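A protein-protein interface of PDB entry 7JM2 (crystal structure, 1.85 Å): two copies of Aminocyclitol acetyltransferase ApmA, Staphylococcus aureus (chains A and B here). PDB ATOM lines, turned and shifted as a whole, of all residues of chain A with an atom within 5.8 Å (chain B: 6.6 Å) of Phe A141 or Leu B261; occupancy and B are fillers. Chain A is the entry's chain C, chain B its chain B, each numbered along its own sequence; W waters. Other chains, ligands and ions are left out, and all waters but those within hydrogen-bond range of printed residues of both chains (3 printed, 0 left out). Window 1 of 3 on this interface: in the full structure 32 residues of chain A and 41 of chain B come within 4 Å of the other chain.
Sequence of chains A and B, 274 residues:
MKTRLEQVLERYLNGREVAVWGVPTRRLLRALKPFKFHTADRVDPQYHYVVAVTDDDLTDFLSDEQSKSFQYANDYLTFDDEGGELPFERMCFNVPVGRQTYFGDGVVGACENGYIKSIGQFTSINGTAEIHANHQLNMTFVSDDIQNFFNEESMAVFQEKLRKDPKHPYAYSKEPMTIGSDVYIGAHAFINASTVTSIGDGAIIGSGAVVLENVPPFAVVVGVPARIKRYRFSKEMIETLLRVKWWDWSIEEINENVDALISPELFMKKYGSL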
ATOM      1  N   GLN A 136       7.576  29.889   1.199  1.00  0.00           N
ATOM      2  CA  GLN A 136       8.288  28.665   0.845  1.00  0.00           C
ATOM      3  C   GLN A 136       7.623  27.995  -0.348  1.00  0.00           C
ATOM      4  O   GLN A 136       6.394  27.987  -0.476  1.00  0.00           O
ATOM      5  CB  GLN A 136       8.335  27.689   2.022  1.00  0.00           C
ATOM      6  CG  GLN A 136       7.016  26.979   2.326  1.00  0.00           C
ATOM      7  CD  GLN A 136       6.024  27.894   3.008  1.00  0.00           C
ATOM      8  OE1 GLN A 136       6.391  28.972   3.481  1.00  0.00           O
ATOM      9  NE2 GLN A 136       4.766  27.472   3.079  1.00  0.00           N
ATOM     10  N   LEU A 137       8.456  27.453  -1.231  1.00  0.00           N
ATOM     11  CA  LEU A 137       8.016  26.761  -2.433  1.00  0.00           C
ATOM     12  C   LEU A 137       8.555  25.340  -2.505  1.00  0.00           C
ATOM     13  O   LEU A 137       8.383  24.673  -3.533  1.00  0.00           O
ATOM     14  CB  LEU A 137       8.445  27.543  -3.679  1.00  0.00           C
ATOM     15  CG  LEU A 137       7.850  28.945  -3.821  1.00  0.00           C
ATOM     16  CD1 LEU A 137       8.703  29.791  -4.767  1.00  0.00           C
ATOM     17  CD2 LEU A 137       6.401  28.859  -4.304  1.00  0.00           C
ATOM     18  N   MET A 139       7.898  23.025   0.052  1.00  0.00           N
ATOM     19  CA  MET A 139       7.090  22.201   0.930  1.00  0.00           C
ATOM     20  C   MET A 139       5.821  21.774   0.196  1.00  0.00           C
ATOM     21  O   MET A 139       5.558  22.180  -0.943  1.00  0.00           O
ATOM     22  CB  MET A 139       6.769  22.952   2.229  1.00  0.00           C
ATOM     23  CG  MET A 139       8.023  23.407   2.968  1.00  0.00           C
ATOM     24  SD  MET A 139       7.725  24.126   4.590  1.00  0.00           S
ATOM     25  CE  MET A 139       9.381  24.727   4.941  1.00  0.00           C
ATOM     26  N   THR A 140       5.022  20.948   0.871  1.00  0.00           N
ATOM     27  CA  THR A 140       3.752  20.535   0.290  1.00  0.00           C
ATOM     28  C   THR A 140       2.783  21.704   0.177  1.00  0.00           C
ATOM     29  O   THR A 140       2.018  21.775  -0.796  1.00  0.00           O
ATOM     30  CB  THR A 140       3.154  19.402   1.119  1.00  0.00           C
ATOM     31  OG1 THR A 140       4.141  18.373   1.283  1.00  0.00           O
ATOM     32  CG2 THR A 140       1.931  18.826   0.446  1.00  0.00           C
ATOM     33  N   PHE A 141       2.829  22.643   1.132  1.00  0.00           N
ATOM     34  CA  PHE A 141       1.950  23.808   1.197  1.00  0.00           C
ATOM     35  C   PHE A 141       2.708  25.100   0.899  1.00  0.00           C
ATOM     36  O   PHE A 141       3.923  25.195   1.102  1.00  0.00           O
ATOM     37  CB  PHE A 141       1.294  23.921   2.587  1.00  0.00           C
ATOM     38  CG  PHE A 141       2.284  24.029   3.730  1.00  0.00           C
ATOM     39  CD1 PHE A 141       2.878  22.899   4.262  1.00  0.00           C
ATOM     40  CD2 PHE A 141       2.603  25.258   4.275  1.00  0.00           C
ATOM     41  CE1 PHE A 141       3.785  22.995   5.312  1.00  0.00           C
ATOM     42  CE2 PHE A 141       3.516  25.361   5.312  1.00  0.00           C
ATOM     43  CZ  PHE A 141       4.102  24.232   5.835  1.00  0.00           C
ATOM     44  N   VAL A 142       1.967  26.105   0.435  1.00  0.00           N
ATOM     45  CA  VAL A 142       2.507  27.442   0.199  1.00  0.00           C
ATOM     46  C   VAL A 142       1.990  28.453   1.208  1.00  0.00           C
ATOM     47  O   VAL A 142       2.567  29.547   1.325  1.00  0.00           O
ATOM     48  CB  VAL A 142       2.217  27.910  -1.248  1.00  0.00           C
ATOM     49  CG1 VAL A 142       0.760  28.317  -1.403  1.00  0.00           C
ATOM     50  CG2 VAL A 142       3.140  29.057  -1.665  1.00  0.00           C
ATOM     51  N   SER A 143       0.953  28.106   1.967  1.00  0.00           N
ATOM     52  CA  SER A 143       0.387  28.953   3.010  1.00  0.00           C
ATOM     53  C   SER A 143       1.436  29.385   4.036  1.00  0.00           C
ATOM     54  O   SER A 143       2.333  28.621   4.397  1.00  0.00           O
ATOM     55  CB  SER A 143      -0.727  28.181   3.724  1.00  0.00           C
ATOM     56  OG  SER A 143      -1.168  28.858   4.880  1.00  0.00           O
ATOM     57  N   ASP A 144       1.298  30.614   4.539  1.00  0.00           N
ATOM     58  CA  ASP A 144       2.073  30.988   5.720  1.00  0.00           C
ATOM     59  C   ASP A 144       1.287  30.813   7.007  1.00  0.00           C
ATOM     60  O   ASP A 144       1.849  30.357   8.013  1.00  0.00           O
ATOM     61  CB  ASP A 144       2.600  32.434   5.631  1.00  0.00           C
ATOM     62  CG  ASP A 144       1.499  33.463   5.464  1.00  0.00           C
ATOM     63  OD1 ASP A 144       0.514  33.160   4.762  1.00  0.00           O
ATOM     64  OD2 ASP A 144       1.642  34.598   5.986  1.00  0.00           O
ATOM     65  N   ILE A 146      -0.970  28.752   8.000  1.00  0.00           N
ATOM     66  CA  ILE A 146      -1.090  27.414   8.575  1.00  0.00           C
ATOM     67  C   ILE A 146      -0.216  27.287   9.819  1.00  0.00           C
ATOM     68  O   ILE A 146      -0.570  26.580  10.778  1.00  0.00           O
ATOM     69  CB  ILE A 146      -0.742  26.357   7.511  1.00  0.00           C
ATOM     70  CG1 ILE A 146      -0.899  24.942   8.076  1.00  0.00           C
ATOM     71  CG2 ILE A 146       0.667  26.584   6.969  1.00  0.00           C
ATOM     72  CD1 ILE A 146      -0.591  23.873   7.066  1.00  0.00           C
ATOM     73  N   PHE A 150       0.442  25.472  14.214  1.00  0.00           N
ATOM     74  CA  PHE A 150       1.582  24.623  14.556  1.00  0.00           C
ATOM     75  C   PHE A 150       1.887  24.725  16.042  1.00  0.00           C
ATOM     76  O   PHE A 150       2.123  25.820  16.563  1.00  0.00           O
ATOM     77  CB  PHE A 150       2.831  25.030  13.768  1.00  0.00           C
ATOM     78  CG  PHE A 150       2.802  24.653  12.313  1.00  0.00           C
ATOM     79  CD1 PHE A 150       1.829  23.812  11.813  1.00  0.00           C
ATOM     80  CD2 PHE A 150       3.766  25.145  11.446  1.00  0.00           C
ATOM     81  CE1 PHE A 150       1.815  23.470  10.457  1.00  0.00           C
ATOM     82  CE2 PHE A 150       3.756  24.808  10.100  1.00  0.00           C
ATOM     83  CZ  PHE A 150       2.777  23.972   9.608  1.00  0.00           C
ATOM     84  N   PHE A 158       9.241  23.449  10.951  1.00  0.00           N
ATOM     85  CA  PHE A 158       8.981  24.344   9.831  1.00  0.00           C
ATOM     86  C   PHE A 158      10.060  25.412   9.736  1.00  0.00           C
ATOM     87  O   PHE A 158      10.576  25.698   8.647  1.00  0.00           O
ATOM     88  CB  PHE A 158       7.589  24.953  10.021  1.00  0.00           C
ATOM     89  CG  PHE A 158       7.210  25.990   9.014  1.00  0.00           C
ATOM     90  CD1 PHE A 158       7.165  25.693   7.664  1.00  0.00           C
ATOM     91  CD2 PHE A 158       6.832  27.258   9.432  1.00  0.00           C
ATOM     92  CE1 PHE A 158       6.780  26.657   6.733  1.00  0.00           C
ATOM     93  CE2 PHE A 158       6.447  28.223   8.522  1.00  0.00           C
ATOM     94  CZ  PHE A 158       6.425  27.927   7.167  1.00  0.00           C
ATOM     95  N   PHE B 122      -6.432  28.014   4.126  1.00  0.00           N
ATOM     96  CA  PHE B 122      -4.988  28.290   4.051  1.00  0.00           C
ATOM     97  C   PHE B 122      -4.613  28.964   2.734  1.00  0.00           C
ATOM     98  O   PHE B 122      -3.623  28.610   2.089  1.00  0.00           O
ATOM     99  CB  PHE B 122      -4.177  27.009   4.257  1.00  0.00           C
ATOM    100  CG  PHE B 122      -4.580  26.258   5.481  1.00  0.00           C
ATOM    101  CD1 PHE B 122      -4.208  26.715   6.734  1.00  0.00           C
ATOM    102  CD2 PHE B 122      -5.356  25.109   5.382  1.00  0.00           C
ATOM    103  CE1 PHE B 122      -4.599  26.049   7.865  1.00  0.00           C
ATOM    104  CE2 PHE B 122      -5.749  24.424   6.533  1.00  0.00           C
ATOM    105  CZ  PHE B 122      -5.371  24.891   7.759  1.00  0.00           C
ATOM    106  N   ASP B 182      -4.912  26.376  -0.227  1.00  0.00           N
ATOM    107  CA  ASP B 182      -3.459  26.464  -0.406  1.00  0.00           C
ATOM    108  C   ASP B 182      -3.100  27.261  -1.661  1.00  0.00           C
ATOM    109  O   ASP B 182      -2.144  26.953  -2.379  1.00  0.00           O
ATOM    110  CB  ASP B 182      -2.824  25.069  -0.424  1.00  0.00           C
ATOM    111  CG  ASP B 182      -1.311  25.109  -0.290  1.00  0.00           C
ATOM    112  OD1 ASP B 182      -0.797  25.881   0.553  1.00  0.00           O
ATOM    113  OD2 ASP B 182      -0.639  24.357  -1.034  1.00  0.00           O
ATOM    114  N   ARG B 232       3.469  23.074  -9.475  1.00  0.00           N
ATOM    115  CA  ARG B 232       4.198  22.901  -8.220  1.00  0.00           C
ATOM    116  C   ARG B 232       4.636  21.460  -8.004  1.00  0.00           C
ATOM    117  O   ARG B 232       5.685  21.218  -7.395  1.00  0.00           O
ATOM    118  CB  ARG B 232       3.344  23.357  -7.045  1.00  0.00           C
ATOM    119  CG  ARG B 232       3.118  24.850  -6.996  1.00  0.00           C
ATOM    120  CD  ARG B 232       2.059  25.195  -5.972  1.00  0.00           C
ATOM    121  NE  ARG B 232       2.410  24.723  -4.632  1.00  0.00           N
ATOM    122  CZ  ARG B 232       1.565  24.715  -3.604  1.00  0.00           C
ATOM    123  NH1 ARG B 232       0.314  25.160  -3.762  1.00  0.00           N
ATOM    124  NH2 ARG B 232       1.965  24.264  -2.420  1.00  0.00           N
ATOM    125  N   PHE B 233       3.851  20.497  -8.475  1.00  0.00           N
ATOM    126  CA  PHE B 233       4.132  19.091  -8.229  1.00  0.00           C
ATOM    127  C   PHE B 233       3.858  18.309  -9.498  1.00  0.00           C
ATOM    128  O   PHE B 233       3.297  18.833 -10.468  1.00  0.00           O
ATOM    129  CB  PHE B 233       3.289  18.532  -7.071  1.00  0.00           C
ATOM    130  CG  PHE B 233       3.391  19.334  -5.807  1.00  0.00           C
ATOM    131  CD1 PHE B 233       2.379  20.210  -5.447  1.00  0.00           C
ATOM    132  CD2 PHE B 233       4.511  19.226  -4.988  1.00  0.00           C
ATOM    133  CE1 PHE B 233       2.471  20.959  -4.293  1.00  0.00           C
ATOM    134  CE2 PHE B 233       4.613  19.972  -3.838  1.00  0.00           C
ATOM    135  CZ  PHE B 233       3.593  20.838  -3.484  1.00  0.00           C
ATOM    136  N   TRP B 246      -5.394  17.789   2.624  1.00  0.00           N
ATOM    137  CA  TRP B 246      -4.868  18.114   3.948  1.00  0.00           C
ATOM    138  C   TRP B 246      -5.411  19.448   4.458  1.00  0.00           C
ATOM    139  O   TRP B 246      -5.449  19.667   5.676  1.00  0.00           O
ATOM    140  CB  TRP B 246      -3.328  18.130   3.938  1.00  0.00           C
ATOM    141  CG  TRP B 246      -2.752  19.210   3.075  1.00  0.00           C
ATOM    142  CD1 TRP B 246      -2.252  19.070   1.815  1.00  0.00           C
ATOM    143  CD2 TRP B 246      -2.647  20.611   3.396  1.00  0.00           C
ATOM    144  NE1 TRP B 246      -1.848  20.295   1.328  1.00  0.00           N
ATOM    145  CE2 TRP B 246      -2.074  21.253   2.281  1.00  0.00           C
ATOM    146  CE3 TRP B 246      -2.975  21.379   4.521  1.00  0.00           C
ATOM    147  CZ2 TRP B 246      -1.827  22.632   2.252  1.00  0.00           C
ATOM    148  CZ3 TRP B 246      -2.725  22.747   4.493  1.00  0.00           C
ATOM    149  CH2 TRP B 246      -2.160  23.357   3.367  1.00  0.00           C
ATOM    150  N   TRP B 247      -5.830  20.346   3.562  1.00  0.00           N
ATOM    151  CA  TRP B 247      -6.374  21.631   3.984  1.00  0.00           C
ATOM    152  C   TRP B 247      -7.694  21.510   4.733  1.00  0.00           C
ATOM    153  O   TRP B 247      -8.151  22.501   5.313  1.00  0.00           O
ATOM    154  CB  TRP B 247      -6.573  22.551   2.777  1.00  0.00           C
ATOM    155  CG  TRP B 247      -7.125  21.862   1.565  1.00  0.00           C
ATOM    156  CD1 TRP B 247      -8.433  21.567   1.307  1.00  0.00           C
ATOM    157  CD2 TRP B 247      -6.381  21.406   0.431  1.00  0.00           C
ATOM    158  NE1 TRP B 247      -8.548  20.942   0.085  1.00  0.00           N
ATOM    159  CE2 TRP B 247      -7.303  20.831  -0.472  1.00  0.00           C
ATOM    160  CE3 TRP B 247      -5.023  21.413   0.095  1.00  0.00           C
ATOM    161  CZ2 TRP B 247      -6.910  20.288  -1.696  1.00  0.00           C
ATOM    162  CZ3 TRP B 247      -4.635  20.854  -1.109  1.00  0.00           C
ATOM    163  CH2 TRP B 247      -5.575  20.308  -1.992  1.00  0.00           C
ATOM    164  N   TRP B 249      -7.890  19.115   7.072  1.00  0.00           N
ATOM    165  CA  TRP B 249      -7.494  18.385   8.274  1.00  0.00           C
ATOM    166  C   TRP B 249      -7.803  19.191   9.530  1.00  0.00           C
ATOM    167  O   TRP B 249      -7.859  20.423   9.509  1.00  0.00           O
ATOM    168  CB  TRP B 249      -6.000  18.073   8.253  1.00  0.00           C
ATOM    169  CG  TRP B 249      -5.629  16.907   7.417  1.00  0.00           C
ATOM    170  CD1 TRP B 249      -6.475  15.999   6.845  1.00  0.00           C
ATOM    171  CD2 TRP B 249      -4.307  16.521   7.037  1.00  0.00           C
ATOM    172  NE1 TRP B 249      -5.756  15.066   6.142  1.00  0.00           N
ATOM    173  CE2 TRP B 249      -4.421  15.365   6.241  1.00  0.00           C
ATOM    174  CE3 TRP B 249      -3.034  17.044   7.293  1.00  0.00           C
ATOM    175  CZ2 TRP B 249      -3.311  14.716   5.703  1.00  0.00           C
ATOM    176  CZ3 TRP B 249      -1.934  16.398   6.763  1.00  0.00           C
ATOM    177  CH2 TRP B 249      -2.079  15.246   5.975  1.00  0.00           C
ATOM    178  N   GLU B 253      -4.594  16.738  13.296  1.00  0.00           N
ATOM    179  CA  GLU B 253      -4.002  16.016  12.175  1.00  0.00           C
ATOM    180  C   GLU B 253      -2.882  16.814  11.525  1.00  0.00           C
ATOM    181  O   GLU B 253      -1.878  16.238  11.091  1.00  0.00           O
ATOM    182  CB  GLU B 253      -5.077  15.669  11.149  1.00  0.00           C
ATOM    183  CG  GLU B 253      -6.054  14.622  11.639  1.00  0.00           C
ATOM    184  CD  GLU B 253      -7.326  14.593  10.821  1.00  0.00           C
ATOM    185  OE1 GLU B 253      -7.739  15.667  10.329  1.00  0.00           O
ATOM    186  OE2 GLU B 253      -7.913  13.499  10.681  1.00  0.00           O
ATOM    187  N   ILE B 254      -3.041  18.136  11.431  1.00  0.00           N
ATOM    188  CA  ILE B 254      -1.986  18.966  10.856  1.00  0.00           C
ATOM    189  C   ILE B 254      -0.675  18.762  11.614  1.00  0.00           C
ATOM    190  O   ILE B 254       0.375  18.516  11.013  1.00  0.00           O
ATOM    191  CB  ILE B 254      -2.416  20.443  10.839  1.00  0.00           C
ATOM    192  CG1 ILE B 254      -3.499  20.673   9.782  1.00  0.00           C
ATOM    193  CG2 ILE B 254      -1.225  21.355  10.554  1.00  0.00           C
ATOM    194  CD1 ILE B 254      -4.009  22.107   9.739  1.00  0.00           C
ATOM    195  N   ASN B 255      -0.718  18.822  12.946  1.00  0.00           N
ATOM    196  CA  ASN B 255       0.516  18.647  13.708  1.00  0.00           C
ATOM    197  C   ASN B 255       1.011  17.206  13.657  1.00  0.00           C
ATOM    198  O   ASN B 255       2.221  16.968  13.583  1.00  0.00           O
ATOM    199  CB  ASN B 255       0.319  19.104  15.152  1.00  0.00           C
ATOM    200  CG  ASN B 255       0.318  20.610  15.273  1.00  0.00           C
ATOM    201  OD1 ASN B 255       1.348  21.258  15.087  1.00  0.00           O
ATOM    202  ND2 ASN B 255      -0.842  21.182  15.571  1.00  0.00           N
ATOM    203  N   ASN B 257       0.878  15.183  11.229  1.00  0.00           N
ATOM    204  CA  ASN B 257       1.473  14.948   9.919  1.00  0.00           C
ATOM    205  C   ASN B 257       2.326  16.119   9.444  1.00  0.00           C
ATOM    206  O   ASN B 257       2.423  16.362   8.238  1.00  0.00           O
ATOM    207  CB  ASN B 257       0.385  14.649   8.895  1.00  0.00           C
ATOM    208  CG  ASN B 257      -0.532  13.545   9.346  1.00  0.00           C
ATOM    209  OD1 ASN B 257      -0.089  12.569   9.943  1.00  0.00           O
ATOM    210  ND2 ASN B 257      -1.825  13.704   9.094  1.00  0.00           N
ATOM    211  N   VAL B 258       2.960  16.842  10.375  1.00  0.00           N
ATOM    212  CA  VAL B 258       3.767  17.999   9.994  1.00  0.00           C
ATOM    213  C   VAL B 258       4.884  17.591   9.037  1.00  0.00           C
ATOM    214  O   VAL B 258       5.197  18.314   8.085  1.00  0.00           O
ATOM    215  CB  VAL B 258       4.311  18.717  11.247  1.00  0.00           C
ATOM    216  CG1 VAL B 258       5.410  17.899  11.940  1.00  0.00           C
ATOM    217  CG2 VAL B 258       4.832  20.102  10.866  1.00  0.00           C
ATOM    218  N   ASP B 259       5.463  16.409   9.236  1.00  0.00           N
ATOM    219  CA  ASP B 259       6.559  15.986   8.371  1.00  0.00           C
ATOM    220  C   ASP B 259       6.080  15.768   6.940  1.00  0.00           C
ATOM    221  O   ASP B 259       6.768  16.153   5.987  1.00  0.00           O
ATOM    222  CB  ASP B 259       7.215  14.722   8.930  1.00  0.00           C
ATOM    223  CG  ASP B 259       7.983  14.987  10.219  1.00  0.00           C
ATOM    224  OD1 ASP B 259       8.784  15.945  10.253  1.00  0.00           O
ATOM    225  OD2 ASP B 259       7.792  14.237  11.197  1.00  0.00           O
ATOM    226  N   ALA B 260       4.896  15.172   6.774  1.00  0.00           N
ATOM    227  CA  ALA B 260       4.318  15.006   5.448  1.00  0.00           C
ATOM    228  C   ALA B 260       3.971  16.347   4.812  1.00  0.00           C
ATOM    229  O   ALA B 260       4.067  16.496   3.592  1.00  0.00           O
ATOM    230  CB  ALA B 260       3.073  14.125   5.524  1.00  0.00           C
ATOM    231  N   LEU B 261       3.567  17.330   5.614  1.00  0.00           N
ATOM    232  CA  LEU B 261       3.299  18.650   5.056  1.00  0.00           C
ATOM    233  C   LEU B 261       4.588  19.359   4.663  1.00  0.00           C
ATOM    234  O   LEU B 261       4.618  20.120   3.693  1.00  0.00           O
ATOM    235  CB  LEU B 261       2.513  19.489   6.064  1.00  0.00           C
ATOM    236  CG  LEU B 261       1.031  19.124   6.229  1.00  0.00           C
ATOM    237  CD1 LEU B 261       0.362  19.982   7.296  1.00  0.00           C
ATOM    238  CD2 LEU B 261       0.301  19.257   4.901  1.00  0.00           C
ATOM    239  N   ILE B 262       5.672  19.106   5.383  1.00  0.00           N
ATOM    240  CA  ILE B 262       6.871  19.884   5.136  1.00  0.00           C
ATOM    241  C   ILE B 262       7.696  19.297   3.996  1.00  0.00           C
ATOM    242  O   ILE B 262       8.365  20.039   3.270  1.00  0.00           O
ATOM    243  CB  ILE B 262       7.627  19.995   6.471  1.00  0.00           C
ATOM    244  CG1 ILE B 262       7.110  21.226   7.228  1.00  0.00           C
ATOM    245  CG2 ILE B 262       9.150  19.967   6.292  1.00  0.00           C
ATOM    246  CD1 ILE B 262       7.532  21.309   8.637  1.00  0.00           C
ATOM    247  N   SER B 263       7.641  17.984   3.787  1.00  0.00           N
ATOM    248  CA  SER B 263       8.436  17.340   2.741  1.00  0.00           C
ATOM    249  C   SER B 263       7.492  16.672   1.749  1.00  0.00           C
ATOM    250  O   SER B 263       6.788  15.709   2.116  1.00  0.00           O
ATOM    251  CB  SER B 263       9.408  16.320   3.343  1.00  0.00           C
ATOM    252  OG  SER B 263       9.685  15.260   2.441  1.00  0.00           O
ATOM    253  N   PRO B 264       7.404  17.155   0.506  1.00  0.00           N
ATOM    254  CA  PRO B 264       6.525  16.487  -0.467  1.00  0.00           C
ATOM    255  C   PRO B 264       6.885  15.035  -0.705  1.00  0.00           C
ATOM    256  O   PRO B 264       5.991  14.198  -0.880  1.00  0.00           O
ATOM    257  CB  PRO B 264       6.706  17.333  -1.731  1.00  0.00           C
ATOM    258  CG  PRO B 264       7.122  18.663  -1.225  1.00  0.00           C
ATOM    259  CD  PRO B 264       7.971  18.405  -0.028  1.00  0.00           C
ATOM    260  N   LEU B 266       7.948  12.873   1.445  1.00  0.00           N
ATOM    261  CA  LEU B 266       7.288  12.104   2.496  1.00  0.00           C
ATOM    262  C   LEU B 266       5.771  12.107   2.322  1.00  0.00           C
ATOM    263  O   LEU B 266       5.100  11.148   2.719  1.00  0.00           O
ATOM    264  CB  LEU B 266       7.678  12.657   3.870  1.00  0.00           C
ATOM    265  CG  LEU B 266       7.563  11.784   5.130  1.00  0.00           C
ATOM    266  CD1 LEU B 266       8.429  12.373   6.241  1.00  0.00           C
ATOM    267  CD2 LEU B 266       6.127  11.620   5.631  1.00  0.00           C
ATOM    268  N   PHE B 267       5.212  13.175   1.745  1.00  0.00           N
ATOM    269  CA  PHE B 267       3.778  13.186   1.481  1.00  0.00           C
ATOM    270  C   PHE B 267       3.387  12.072   0.513  1.00  0.00           C
ATOM    271  O   PHE B 267       2.362  11.410   0.698  1.00  0.00           O
ATOM    272  CB  PHE B 267       3.351  14.545   0.932  1.00  0.00           C
ATOM    273  CG  PHE B 267       1.872  14.745   0.920  1.00  0.00           C
ATOM    274  CD1 PHE B 267       1.126  14.427  -0.203  1.00  0.00           C
ATOM    275  CD2 PHE B 267       1.220  15.249   2.036  1.00  0.00           C
ATOM    276  CE1 PHE B 267      -0.241  14.616  -0.211  1.00  0.00           C
ATOM    277  CE2 PHE B 267      -0.145  15.442   2.031  1.00  0.00           C
ATOM    278  CZ  PHE B 267      -0.875  15.128   0.907  1.00  0.00           C
ATOM    279  N   TYR B 271       1.021   8.899   1.286  1.00  0.00           N
ATOM    280  CA  TYR B 271      -0.292   9.047   0.677  1.00  0.00           C
ATOM    281  C   TYR B 271      -0.344   8.675  -0.799  1.00  0.00           C
ATOM    282  O   TYR B 271      -1.444   8.461  -1.318  1.00  0.00           O
ATOM    283  CB  TYR B 271      -0.802  10.496   0.836  1.00  0.00           C
ATOM    284  CG  TYR B 271      -0.987  10.923   2.279  1.00  0.00           C
ATOM    285  CD1 TYR B 271      -2.009  10.390   3.049  1.00  0.00           C
ATOM    286  CD2 TYR B 271      -0.134  11.852   2.872  1.00  0.00           C
ATOM    287  CE1 TYR B 271      -2.188  10.765   4.361  1.00  0.00           C
ATOM    288  CE2 TYR B 271      -0.307  12.235   4.189  1.00  0.00           C
ATOM    289  CZ  TYR B 271      -1.337  11.683   4.931  1.00  0.00           C
ATOM    290  OH  TYR B 271      -1.525  12.042   6.245  1.00  0.00           O
HETATM  291  O   HOH W   1      -1.588  30.027   0.777  1.00  0.00           O
HETATM  292  O   HOH W   2       5.017  24.070  -3.476  1.00  0.00           O
HETATM  293  O   HOH W   3      -0.828  21.676  -1.158  1.00  0.00           O
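Water W3 lies within hydrogen-bond range of OD2 of Asp B182 (2.7 Å), O of Thr A140 (2.9 Å) and NE1 of Trp B246 (3.0 Å).
Water W1 bridges O of Phe B122 and N of Ser A143.
Water W2 lies within hydrogen-bond range of the guanidinium group of Arg B232 (2.9 Å), the backbone carbonyl oxygen of Met A139 (3.2 Å) and the backbone carbonyl oxygen of Leu A137 (3.4 Å).
Phe A141 touches just these residues of chain B: Asp B182, Arg B232, Trp B246 and Leu B261.
Of the printed residues of chain B, Ser A143 touches Phe B122 (3.4 Å) and Asp B182 (3.2 Å).
Asp A144 touches none of the printed residues of chain B.
Of the printed residues of chain A, Asp B182 touches Thr A140, Phe A141, Val A142 and Ser A143.
Glu B253 touches none of the printed residues of chain A.
Of the printed residues of chain A, Ala B260 touches Thr A140 (3.0 Å).
Of the printed residues of chain A, Leu B261 touches Met A139, Thr A140 and Phe A141.
Of the printed residues of chain A, Phe B267 touches Thr A140.
The nearest residue of chain B that does not touch Phe A141 is Ile B262 (4.2 Å).
The nearest printed residue of chain A that does not touch Leu B261 is Ile A146 (4.01 Å).
NH2 of Arg B232 sits close to N of Val A142.
O of Thr A140 sits at hydrogen-bond distance from NH2 of Arg B232 (3.0 Å).
OD1 of Asp B182 sits at hydrogen-bond distance from N of Ser A143 (3.2 Å).
The backbone NH of Thr A140 is in hydrogen-bond range of the backbone carbonyl oxygen of Leu B261 (3.0 Å).
The side-chain carboxylate (OD1) of Asp B182 sits at hydrogen-bond distance from the backbone NH (N) of Val A142.
O of Ala B260 is in hydrogen-bond range of OG1 of Thr A140, at 3.0 Å.
No position is printed for both chains.
Of the 25 pairs that touch across the chains among the printed residues, none has its exchanged pair printed and touching as well.
Among the printed residues, pairs that only touch across the chains: Thr A140 with Phe B233 (3.3 Å), Phe A141 with Leu B261 (3.3 Å), Ser A143 with Phe B122 (3.4 Å), Phe A141 with Trp B246 (3.4 Å), Met A139 with Ile B262 (3.4 Å), Phe A150 with Asn B255 (3.4 Å), Phe A141 with Asp B182 (3.5 Å), Met A139 with Phe B233 (3.5 Å), Phe A141 with Arg B232 (3.5 Å), Thr A140 with Pro B264 (3.5 Å), Ile A146 with Trp B246 (3.5 Å), Phe A158 with Ile B262 (3.6 Å), Ile A146 with Phe B122 (3.6 Å), Met A139 with Pro B264 (3.7 Å), Phe A150 with Ile B254 (3.7 Å), Thr A140 with Asp B182 (3.7 Å), Thr A140 with Ser B263 (3.8 Å), Met A139 with Leu B261 (3.8 Å) and Thr A140 with Phe B267 (3.9 Å).
Of the 11 printed residues of chain A, 8 touch a printed residue of chain B.
Hydrophobic or aromatic side chains of chain A that line the printed part of chain B: Met A139, Phe A141, Val A142, Ile A146, Phe A150 and Phe A158.
Hydrophobic or aromatic side chains of chain B within 4 Å of the printed part of chain A: Phe B122, Phe B233, Trp B246, Ile B254, Leu B261, Ile B262, Pro B264 and Phe B267.
Among the printed residues, 25 pairs touch across the chains.
Among the printed residues, no Asp or Glu carboxylate lies within 4 Å of a Lys or Arg side-chain nitrogen of the other chain.
O of Phe B122 sits close to N of Asp B182 (3.5 Å).
The backbone NH of Ile A146 is in hydrogen-bond range of the side-chain hydroxyl of Ser A143, 3.1 Å away.
O of Ser A143 lies within hydrogen-bond range of NE2 of Gln A136 (3.0 Å).
The side-chain amide nitrogen of Gln A136 is in hydrogen-bond range of the backbone carbonyl oxygen of Phe A141 (3.1 Å).
The side-chain hydroxyl of Ser B263 is in hydrogen-bond range of the backbone NH of Leu B266 (3.1 Å).
The guanidinium group of Arg B232 is in salt-bridge range of the side-chain carboxylate of Asp B182.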
